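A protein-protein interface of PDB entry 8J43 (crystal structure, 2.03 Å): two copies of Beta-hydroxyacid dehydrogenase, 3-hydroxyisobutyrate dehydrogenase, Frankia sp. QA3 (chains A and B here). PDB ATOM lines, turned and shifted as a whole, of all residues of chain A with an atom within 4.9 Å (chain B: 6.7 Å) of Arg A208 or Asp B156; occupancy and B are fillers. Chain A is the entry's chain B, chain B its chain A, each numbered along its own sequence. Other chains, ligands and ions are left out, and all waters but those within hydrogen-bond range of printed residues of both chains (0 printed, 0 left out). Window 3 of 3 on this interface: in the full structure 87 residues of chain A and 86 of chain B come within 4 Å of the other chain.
Of the printed residues of chain B, Val A207 touches Ala B214.
Arg A208 touches three residues of chain B.
Of the printed residues of chain B, Trp A209 touches Met B134.
Ala A212 touches none of the printed residues of chain B.
Pro B131 touches none of the printed residues of chain A.
Of the printed residues of chain A, Met B134 touches Phe A205 (3.5 Å), Arg A208 (3.6 Å) and Trp A209 (3.8 Å).
Printed residues of chain A within 4 Å of Leu B158: Phe A205.
Printed residues of chain A within 4 Å of Ala B214: Val A207.
The nearest printed residue of chain A that does not touch Glu B132 is Ala A212 (6.7 Å).
The backbone carbonyl oxygen of Met B133 lies within hydrogen-bond range of the backbone NH of Asp B156 (2.8 Å).
The backbone NH of Phe B135 sits at hydrogen-bond distance from the backbone carbonyl oxygen of Asp B156 (3.0 Å).
The backbone NH of Tyr B137 sits at hydrogen-bond distance from the backbone carbonyl oxygen of Leu B158 (2.9 Å).
The side-chain hydroxyl of Ser B130 sits close to the backbone NH of Glu B132.
The backbone carbonyl oxygen of Phe B135 lies within hydrogen-bond range of the backbone NH of Leu B158 (2.8 Å).
Met B134 touches Phe A205.
Leu B136 touches Phe A205 (CD2 to CD2, 3.98 Å).
CD1 of Leu B158 touches CE2 of Phe A205, at 3.97 Å.
O of Ala B214 touches CG2 of Val A207 (3.7 Å).
CZ of Arg A208 touches CG of Met B134, 3.6 Å away.
Trp A209 touches Met B134 (N to CE, 3.8 Å).
Printed residues of chain A that touch a printed residue of chain B: Phe A205, Val A207, Arg A208 and Trp A209.
Hydrophobic or aromatic side chains of chain A within 4 Å of the printed part of chain B: Phe A205, Val A207 and Trp A209.
Of the 17 printed residues of chain B, 6 touch a printed residue of chain A.
Printed residues of chain B that touch a printed residue of chain A: Glu B132, Met B134, Leu B136, Asp B156, Leu B158 and Ala B214.
Hydrophobic or aromatic side chains of chain B within 4 Å of the printed part of chain A: Met B134, Leu B136, Leu B158 and Ala B214.
Among the printed residues, 8 pairs touch across the chains.
Among the printed residues, Asp or Glu carboxylates within 4 Å of a Lys or Arg side-chain nitrogen of the other chain: Arg A208 with Asp B156.
The side-chain carboxylate of Asp B156 is in salt-bridge range of the guanidinium group of Arg A208 (3.0 Å).
The backbone carbonyl oxygen (O) of Glu B132 is in hydrogen-bond range of the guanidinium group (NH2) of Arg A208 (2.9 Å).
No position is printed for both chains.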
ATOM      1  N   PRO A 204      21.553   9.528  19.670  1.00  0.00           N
ATOM      2  CA  PRO A 204      22.229   8.427  20.376  1.00  0.00           C
ATOM      3  C   PRO A 204      22.600   8.761  21.836  1.00  0.00           C
ATOM      4  O   PRO A 204      22.622   7.857  22.688  1.00  0.00           O
ATOM      5  CB  PRO A 204      23.490   8.171  19.519  1.00  0.00           C
ATOM      6  CG  PRO A 204      23.089   8.636  18.149  1.00  0.00           C
ATOM      7  CD  PRO A 204      22.207   9.834  18.386  1.00  0.00           C
ATOM      8  N   PHE A 205      22.856  10.031  22.131  1.00  0.00           N
ATOM      9  CA  PHE A 205      23.099  10.463  23.518  1.00  0.00           C
ATOM     10  C   PHE A 205      21.819  10.387  24.332  1.00  0.00           C
ATOM     11  O   PHE A 205      21.849   9.977  25.491  1.00  0.00           O
ATOM     12  CB  PHE A 205      23.676  11.884  23.591  1.00  0.00           C
ATOM     13  CG  PHE A 205      25.056  12.013  23.002  1.00  0.00           C
ATOM     14  CD1 PHE A 205      25.237  12.224  21.638  1.00  0.00           C
ATOM     15  CD2 PHE A 205      26.163  11.963  23.807  1.00  0.00           C
ATOM     16  CE1 PHE A 205      26.510  12.356  21.090  1.00  0.00           C
ATOM     17  CE2 PHE A 205      27.446  12.077  23.270  1.00  0.00           C
ATOM     18  CZ  PHE A 205      27.617  12.291  21.910  1.00  0.00           C
ATOM     19  N   ALA A 206      20.698  10.784  23.721  1.00  0.00           N
ATOM     20  CA  ALA A 206      19.381  10.653  24.347  1.00  0.00           C
ATOM     21  C   ALA A 206      19.040   9.192  24.646  1.00  0.00           C
ATOM     22  O   ALA A 206      18.529   8.885  25.718  1.00  0.00           O
ATOM     23  CB  ALA A 206      18.295  11.282  23.481  1.00  0.00           C
ATOM     24  N   VAL A 207      19.337   8.303  23.706  1.00  0.00           N
ATOM     25  CA  VAL A 207      19.007   6.895  23.864  1.00  0.00           C
ATOM     26  C   VAL A 207      19.788   6.351  25.045  1.00  0.00           C
ATOM     27  O   VAL A 207      19.235   5.733  25.947  1.00  0.00           O
ATOM     28  CB  VAL A 207      19.289   6.097  22.585  1.00  0.00           C
ATOM     29  CG1 VAL A 207      19.168   4.597  22.837  1.00  0.00           C
ATOM     30  CG2 VAL A 207      18.322   6.530  21.487  1.00  0.00           C
ATOM     31  N   ARG A 208      21.081   6.615  25.048  1.00  0.00           N
ATOM     32  CA  ARG A 208      21.949   6.158  26.130  1.00  0.00           C
ATOM     33  C   ARG A 208      21.527   6.724  27.485  1.00  0.00           C
ATOM     34  O   ARG A 208      21.459   6.002  28.472  1.00  0.00           O
ATOM     35  CB  ARG A 208      23.383   6.571  25.823  1.00  0.00           C
ATOM     36  CG  ARG A 208      24.381   6.002  26.789  1.00  0.00           C
ATOM     37  CD  ARG A 208      25.764   5.967  26.200  1.00  0.00           C
ATOM     38  NE  ARG A 208      26.657   5.592  27.265  1.00  0.00           N
ATOM     39  CZ  ARG A 208      27.967   5.771  27.254  1.00  0.00           C
ATOM     40  NH1 ARG A 208      28.576   6.313  26.208  1.00  0.00           N
ATOM     41  NH2 ARG A 208      28.668   5.379  28.306  1.00  0.00           N
ATOM     42  N   TRP A 209      21.229   8.019  27.505  1.00  0.00           N
ATOM     43  CA  TRP A 209      20.715   8.686  28.697  1.00  0.00           C
ATOM     44  C   TRP A 209      19.452   8.013  29.221  1.00  0.00           C
ATOM     45  O   TRP A 209      19.252   7.951  30.426  1.00  0.00           O
ATOM     46  CB  TRP A 209      20.447  10.161  28.379  1.00  0.00           C
ATOM     47  CG  TRP A 209      19.828  11.034  29.458  1.00  0.00           C
ATOM     48  CD1 TRP A 209      18.783  11.884  29.291  1.00  0.00           C
ATOM     49  CD2 TRP A 209      20.249  11.190  30.840  1.00  0.00           C
ATOM     50  NE1 TRP A 209      18.507  12.545  30.465  1.00  0.00           N
ATOM     51  CE2 TRP A 209      19.391  12.144  31.429  1.00  0.00           C
ATOM     52  CE3 TRP A 209      21.258  10.618  31.621  1.00  0.00           C
ATOM     53  CZ2 TRP A 209      19.505  12.536  32.766  1.00  0.00           C
ATOM     54  CZ3 TRP A 209      21.371  11.001  32.953  1.00  0.00           C
ATOM     55  CH2 TRP A 209      20.503  11.955  33.517  1.00  0.00           C
ATOM     56  N   LEU A 210      18.585   7.529  28.328  1.00  0.00           N
ATOM     57  CA  LEU A 210      17.341   6.918  28.783  1.00  0.00           C
ATOM     58  C   LEU A 210      17.569   5.655  29.612  1.00  0.00           C
ATOM     59  O   LEU A 210      16.705   5.273  30.416  1.00  0.00           O
ATOM     60  CB  LEU A 210      16.410   6.629  27.608  1.00  0.00           C
ATOM     61  CG  LEU A 210      15.505   7.801  27.223  1.00  0.00           C
ATOM     62  CD1 LEU A 210      14.791   7.456  25.911  1.00  0.00           C
ATOM     63  CD2 LEU A 210      14.515   8.144  28.349  1.00  0.00           C
ATOM     64  N   THR A 211      18.698   4.983  29.391  1.00  0.00           N
ATOM     65  CA  THR A 211      19.084   3.842  30.235  1.00  0.00           C
ATOM     66  C   THR A 211      19.273   4.289  31.684  1.00  0.00           C
ATOM     67  O   THR A 211      18.713   3.703  32.596  1.00  0.00           O
ATOM     68  CB  THR A 211      20.353   3.144  29.717  1.00  0.00           C
ATOM     69  OG1 THR A 211      20.096   2.640  28.404  1.00  0.00           O
ATOM     70  CG2 THR A 211      20.750   1.978  30.634  1.00  0.00           C
ATOM     71  N   ALA A 212      20.013   5.362  31.886  1.00  0.00           N
ATOM     72  CA  ALA A 212      20.197   5.914  33.238  1.00  0.00           C
ATOM     73  C   ALA A 212      18.894   6.481  33.828  1.00  0.00           C
ATOM     74  O   ALA A 212      18.633   6.359  35.019  1.00  0.00           O
ATOM     75  CB  ALA A 212      21.288   6.970  33.223  1.00  0.00           C
ATOM     76  N   SER B 130      31.307   5.000  37.692  1.00  0.00           N
ATOM     77  CA  SER B 130      30.948   3.966  36.721  1.00  0.00           C
ATOM     78  C   SER B 130      31.257   4.371  35.266  1.00  0.00           C
ATOM     79  O   SER B 130      30.731   5.367  34.765  1.00  0.00           O
ATOM     80  CB  SER B 130      29.473   3.595  36.851  1.00  0.00           C
ATOM     81  OG  SER B 130      29.034   2.994  35.644  1.00  0.00           O
ATOM     82  N   PRO B 131      32.092   3.581  34.569  1.00  0.00           N
ATOM     83  CA  PRO B 131      32.391   3.895  33.166  1.00  0.00           C
ATOM     84  C   PRO B 131      31.203   3.850  32.193  1.00  0.00           C
ATOM     85  O   PRO B 131      31.375   4.229  31.051  1.00  0.00           O
ATOM     86  CB  PRO B 131      33.462   2.855  32.778  1.00  0.00           C
ATOM     87  CG  PRO B 131      33.341   1.760  33.766  1.00  0.00           C
ATOM     88  CD  PRO B 131      32.786   2.361  35.031  1.00  0.00           C
ATOM     89  N   GLU B 132      30.017   3.410  32.617  1.00  0.00           N
ATOM     90  CA  GLU B 132      28.829   3.509  31.762  1.00  0.00           C
ATOM     91  C   GLU B 132      28.178   4.878  31.813  1.00  0.00           C
ATOM     92  O   GLU B 132      27.385   5.197  30.938  1.00  0.00           O
ATOM     93  CB  GLU B 132      27.781   2.447  32.131  1.00  0.00           C
ATOM     94  CG  GLU B 132      28.309   1.020  32.087  1.00  0.00           C
ATOM     95  CD  GLU B 132      28.629   0.562  30.663  1.00  0.00           C
ATOM     96  OE1 GLU B 132      27.676   0.437  29.856  1.00  0.00           O
ATOM     97  OE2 GLU B 132      29.827   0.354  30.346  1.00  0.00           O
ATOM     98  N   MET B 133      28.488   5.684  32.830  1.00  0.00           N
ATOM     99  CA  MET B 133      27.834   6.986  32.965  1.00  0.00           C
ATOM    100  C   MET B 133      28.550   8.071  32.151  1.00  0.00           C
ATOM    101  O   MET B 133      29.761   8.308  32.321  1.00  0.00           O
ATOM    102  CB  MET B 133      27.725   7.398  34.432  1.00  0.00           C
ATOM    103  CG  MET B 133      26.840   6.483  35.247  1.00  0.00           C
ATOM    104  SD  MET B 133      25.158   6.276  34.632  1.00  0.00           S
ATOM    105  CE  MET B 133      24.636   5.065  35.849  1.00  0.00           C
ATOM    106  N   MET B 134      27.783   8.738  31.289  1.00  0.00           N
ATOM    107  CA  MET B 134      28.304   9.797  30.421  1.00  0.00           C
ATOM    108  C   MET B 134      28.658  11.052  31.215  1.00  0.00           C
ATOM    109  O   MET B 134      27.879  11.506  32.050  1.00  0.00           O
ATOM    110  CB  MET B 134      27.270  10.182  29.353  1.00  0.00           C
ATOM    111  CG  MET B 134      26.926   9.079  28.368  1.00  0.00           C
ATOM    112  SD  MET B 134      25.908   9.707  27.024  1.00  0.00           S
ATOM    113  CE  MET B 134      24.403  10.090  27.943  1.00  0.00           C
ATOM    114  N   PHE B 135      29.846  11.588  30.938  1.00  0.00           N
ATOM    115  CA  PHE B 135      30.231  12.932  31.312  1.00  0.00           C
ATOM    116  C   PHE B 135      30.527  13.632  29.989  1.00  0.00           C
ATOM    117  O   PHE B 135      31.408  13.190  29.246  1.00  0.00           O
ATOM    118  CB  PHE B 135      31.486  12.933  32.211  1.00  0.00           C
ATOM    119  CG  PHE B 135      31.215  12.560  33.658  1.00  0.00           C
ATOM    120  CD1 PHE B 135      30.690  11.321  33.985  1.00  0.00           C
ATOM    121  CD2 PHE B 135      31.537  13.435  34.693  1.00  0.00           C
ATOM    122  CE1 PHE B 135      30.457  10.961  35.305  1.00  0.00           C
ATOM    123  CE2 PHE B 135      31.309  13.084  36.026  1.00  0.00           C
ATOM    124  CZ  PHE B 135      30.771  11.848  36.335  1.00  0.00           C
ATOM    125  N   LEU B 136      29.796  14.702  29.688  1.00  0.00           N
ATOM    126  CA  LEU B 136      29.945  15.393  28.407  1.00  0.00           C
ATOM    127  C   LEU B 136      30.810  16.613  28.602  1.00  0.00           C
ATOM    128  O   LEU B 136      30.578  17.374  29.557  1.00  0.00           O
ATOM    129  CB  LEU B 136      28.576  15.817  27.861  1.00  0.00           C
ATOM    130  CG  LEU B 136      27.483  14.740  27.900  1.00  0.00           C
ATOM    131  CD1 LEU B 136      26.147  15.323  27.491  1.00  0.00           C
ATOM    132  CD2 LEU B 136      27.844  13.547  27.043  1.00  0.00           C
ATOM    133  N   TYR B 137      31.789  16.809  27.717  1.00  0.00           N
ATOM    134  CA  TYR B 137      32.745  17.896  27.863  1.00  0.00           C
ATOM    135  C   TYR B 137      32.806  18.747  26.614  1.00  0.00           C
ATOM    136  O   TYR B 137      32.684  18.235  25.496  1.00  0.00           O
ATOM    137  CB  TYR B 137      34.158  17.356  28.159  1.00  0.00           C
ATOM    138  CG  TYR B 137      34.264  16.735  29.520  1.00  0.00           C
ATOM    139  CD1 TYR B 137      34.454  17.522  30.652  1.00  0.00           C
ATOM    140  CD2 TYR B 137      34.145  15.356  29.686  1.00  0.00           C
ATOM    141  CE1 TYR B 137      34.518  16.945  31.922  1.00  0.00           C
ATOM    142  CE2 TYR B 137      34.205  14.781  30.944  1.00  0.00           C
ATOM    143  CZ  TYR B 137      34.393  15.578  32.056  1.00  0.00           C
ATOM    144  OH  TYR B 137      34.450  15.009  33.309  1.00  0.00           O
ATOM    145  N   ARG B 148      42.193  13.430  30.022  1.00  0.00           N
ATOM    146  CA  ARG B 148      41.206  12.360  29.851  1.00  0.00           C
ATOM    147  C   ARG B 148      41.304  11.263  30.911  1.00  0.00           C
ATOM    148  O   ARG B 148      40.295  10.785  31.434  1.00  0.00           O
ATOM    149  CB  ARG B 148      41.344  11.708  28.478  1.00  0.00           C
ATOM    150  CG  ARG B 148      40.138  10.846  28.154  1.00  0.00           C
ATOM    151  CD  ARG B 148      40.357   9.956  26.955  1.00  0.00           C
ATOM    152  NE  ARG B 148      39.139   9.200  26.660  1.00  0.00           N
ATOM    153  CZ  ARG B 148      38.713   8.129  27.332  1.00  0.00           C
ATOM    154  NH1 ARG B 148      39.377   7.661  28.379  1.00  0.00           N
ATOM    155  NH2 ARG B 148      37.592   7.532  26.961  1.00  0.00           N
ATOM    156  N   LEU B 151      39.730  12.345  34.105  1.00  0.00           N
ATOM    157  CA  LEU B 151      38.284  12.419  33.897  1.00  0.00           C
ATOM    158  C   LEU B 151      37.640  11.027  33.830  1.00  0.00           C
ATOM    159  O   LEU B 151      36.518  10.828  34.295  1.00  0.00           O
ATOM    160  CB  LEU B 151      37.959  13.187  32.620  1.00  0.00           C
ATOM    161  CG  LEU B 151      38.473  14.624  32.517  1.00  0.00           C
ATOM    162  CD1 LEU B 151      38.132  15.165  31.138  1.00  0.00           C
ATOM    163  CD2 LEU B 151      37.884  15.508  33.603  1.00  0.00           C
ATOM    164  N   ALA B 152      38.356  10.069  33.244  1.00  0.00           N
ATOM    165  CA  ALA B 152      37.888   8.681  33.148  1.00  0.00           C
ATOM    166  C   ALA B 152      37.641   8.020  34.518  1.00  0.00           C
ATOM    167  O   ALA B 152      36.890   7.045  34.613  1.00  0.00           O
ATOM    168  CB  ALA B 152      38.882   7.840  32.343  1.00  0.00           C
ATOM    169  N   LEU B 154      35.938   9.358  36.767  1.00  0.00           N
ATOM    170  CA  LEU B 154      34.599   9.793  37.178  1.00  0.00           C
ATOM    171  C   LEU B 154      33.489   9.113  36.384  1.00  0.00           C
ATOM    172  O   LEU B 154      32.345   9.007  36.874  1.00  0.00           O
ATOM    173  CB  LEU B 154      34.468  11.305  37.011  1.00  0.00           C
ATOM    174  CG  LEU B 154      35.514  12.138  37.749  1.00  0.00           C
ATOM    175  CD1 LEU B 154      35.374  13.607  37.359  1.00  0.00           C
ATOM    176  CD2 LEU B 154      35.387  11.959  39.269  1.00  0.00           C
ATOM    177  N   GLY B 155      33.829   8.673  35.166  1.00  0.00           N
ATOM    178  CA  GLY B 155      32.877   8.071  34.261  1.00  0.00           C
ATOM    179  C   GLY B 155      33.431   7.978  32.850  1.00  0.00           C
ATOM    180  O   GLY B 155      34.641   7.963  32.660  1.00  0.00           O
ATOM    181  N   ASP B 156      32.541   7.922  31.871  1.00  0.00           N
ATOM    182  CA  ASP B 156      32.909   7.884  30.457  1.00  0.00           C
ATOM    183  C   ASP B 156      33.000   9.307  29.908  1.00  0.00           C
ATOM    184  O   ASP B 156      31.973   9.955  29.693  1.00  0.00           O
ATOM    185  CB  ASP B 156      31.852   7.089  29.673  1.00  0.00           C
ATOM    186  CG  ASP B 156      32.268   6.811  28.247  1.00  0.00           C
ATOM    187  OD1 ASP B 156      33.439   7.038  27.900  1.00  0.00           O
ATOM    188  OD2 ASP B 156      31.412   6.359  27.467  1.00  0.00           O
ATOM    189  N   PRO B 157      34.219   9.803  29.683  1.00  0.00           N
ATOM    190  CA  PRO B 157      34.321  11.193  29.297  1.00  0.00           C
ATOM    191  C   PRO B 157      34.212  11.360  27.790  1.00  0.00           C
ATOM    192  O   PRO B 157      35.037  10.835  27.055  1.00  0.00           O
ATOM    193  CB  PRO B 157      35.708  11.598  29.819  1.00  0.00           C
ATOM    194  CG  PRO B 157      36.489  10.313  29.903  1.00  0.00           C
ATOM    195  CD  PRO B 157      35.540   9.157  29.733  1.00  0.00           C
ATOM    196  N   LEU B 158      33.186  12.075  27.351  1.00  0.00           N
ATOM    197  CA  LEU B 158      32.874  12.247  25.935  1.00  0.00           C
ATOM    198  C   LEU B 158      33.063  13.703  25.541  1.00  0.00           C
ATOM    199  O   LEU B 158      32.340  14.583  26.022  1.00  0.00           O
ATOM    200  CB  LEU B 158      31.421  11.848  25.661  1.00  0.00           C
ATOM    201  CG  LEU B 158      31.050  10.440  26.113  1.00  0.00           C
ATOM    202  CD1 LEU B 158      29.538  10.268  26.123  1.00  0.00           C
ATOM    203  CD2 LEU B 158      31.731   9.413  25.224  1.00  0.00           C
ATOM    204  N   ALA B 214      12.871   4.332  23.145  1.00  0.00           N
ATOM    205  CA  ALA B 214      14.167   4.838  22.698  1.00  0.00           C
ATOM    206  C   ALA B 214      14.369   4.509  21.214  1.00  0.00           C
ATOM    207  O   ALA B 214      14.943   5.290  20.480  1.00  0.00           O
ATOM    208  CB  ALA B 214      15.298   4.256  23.522  1.00  0.00           C
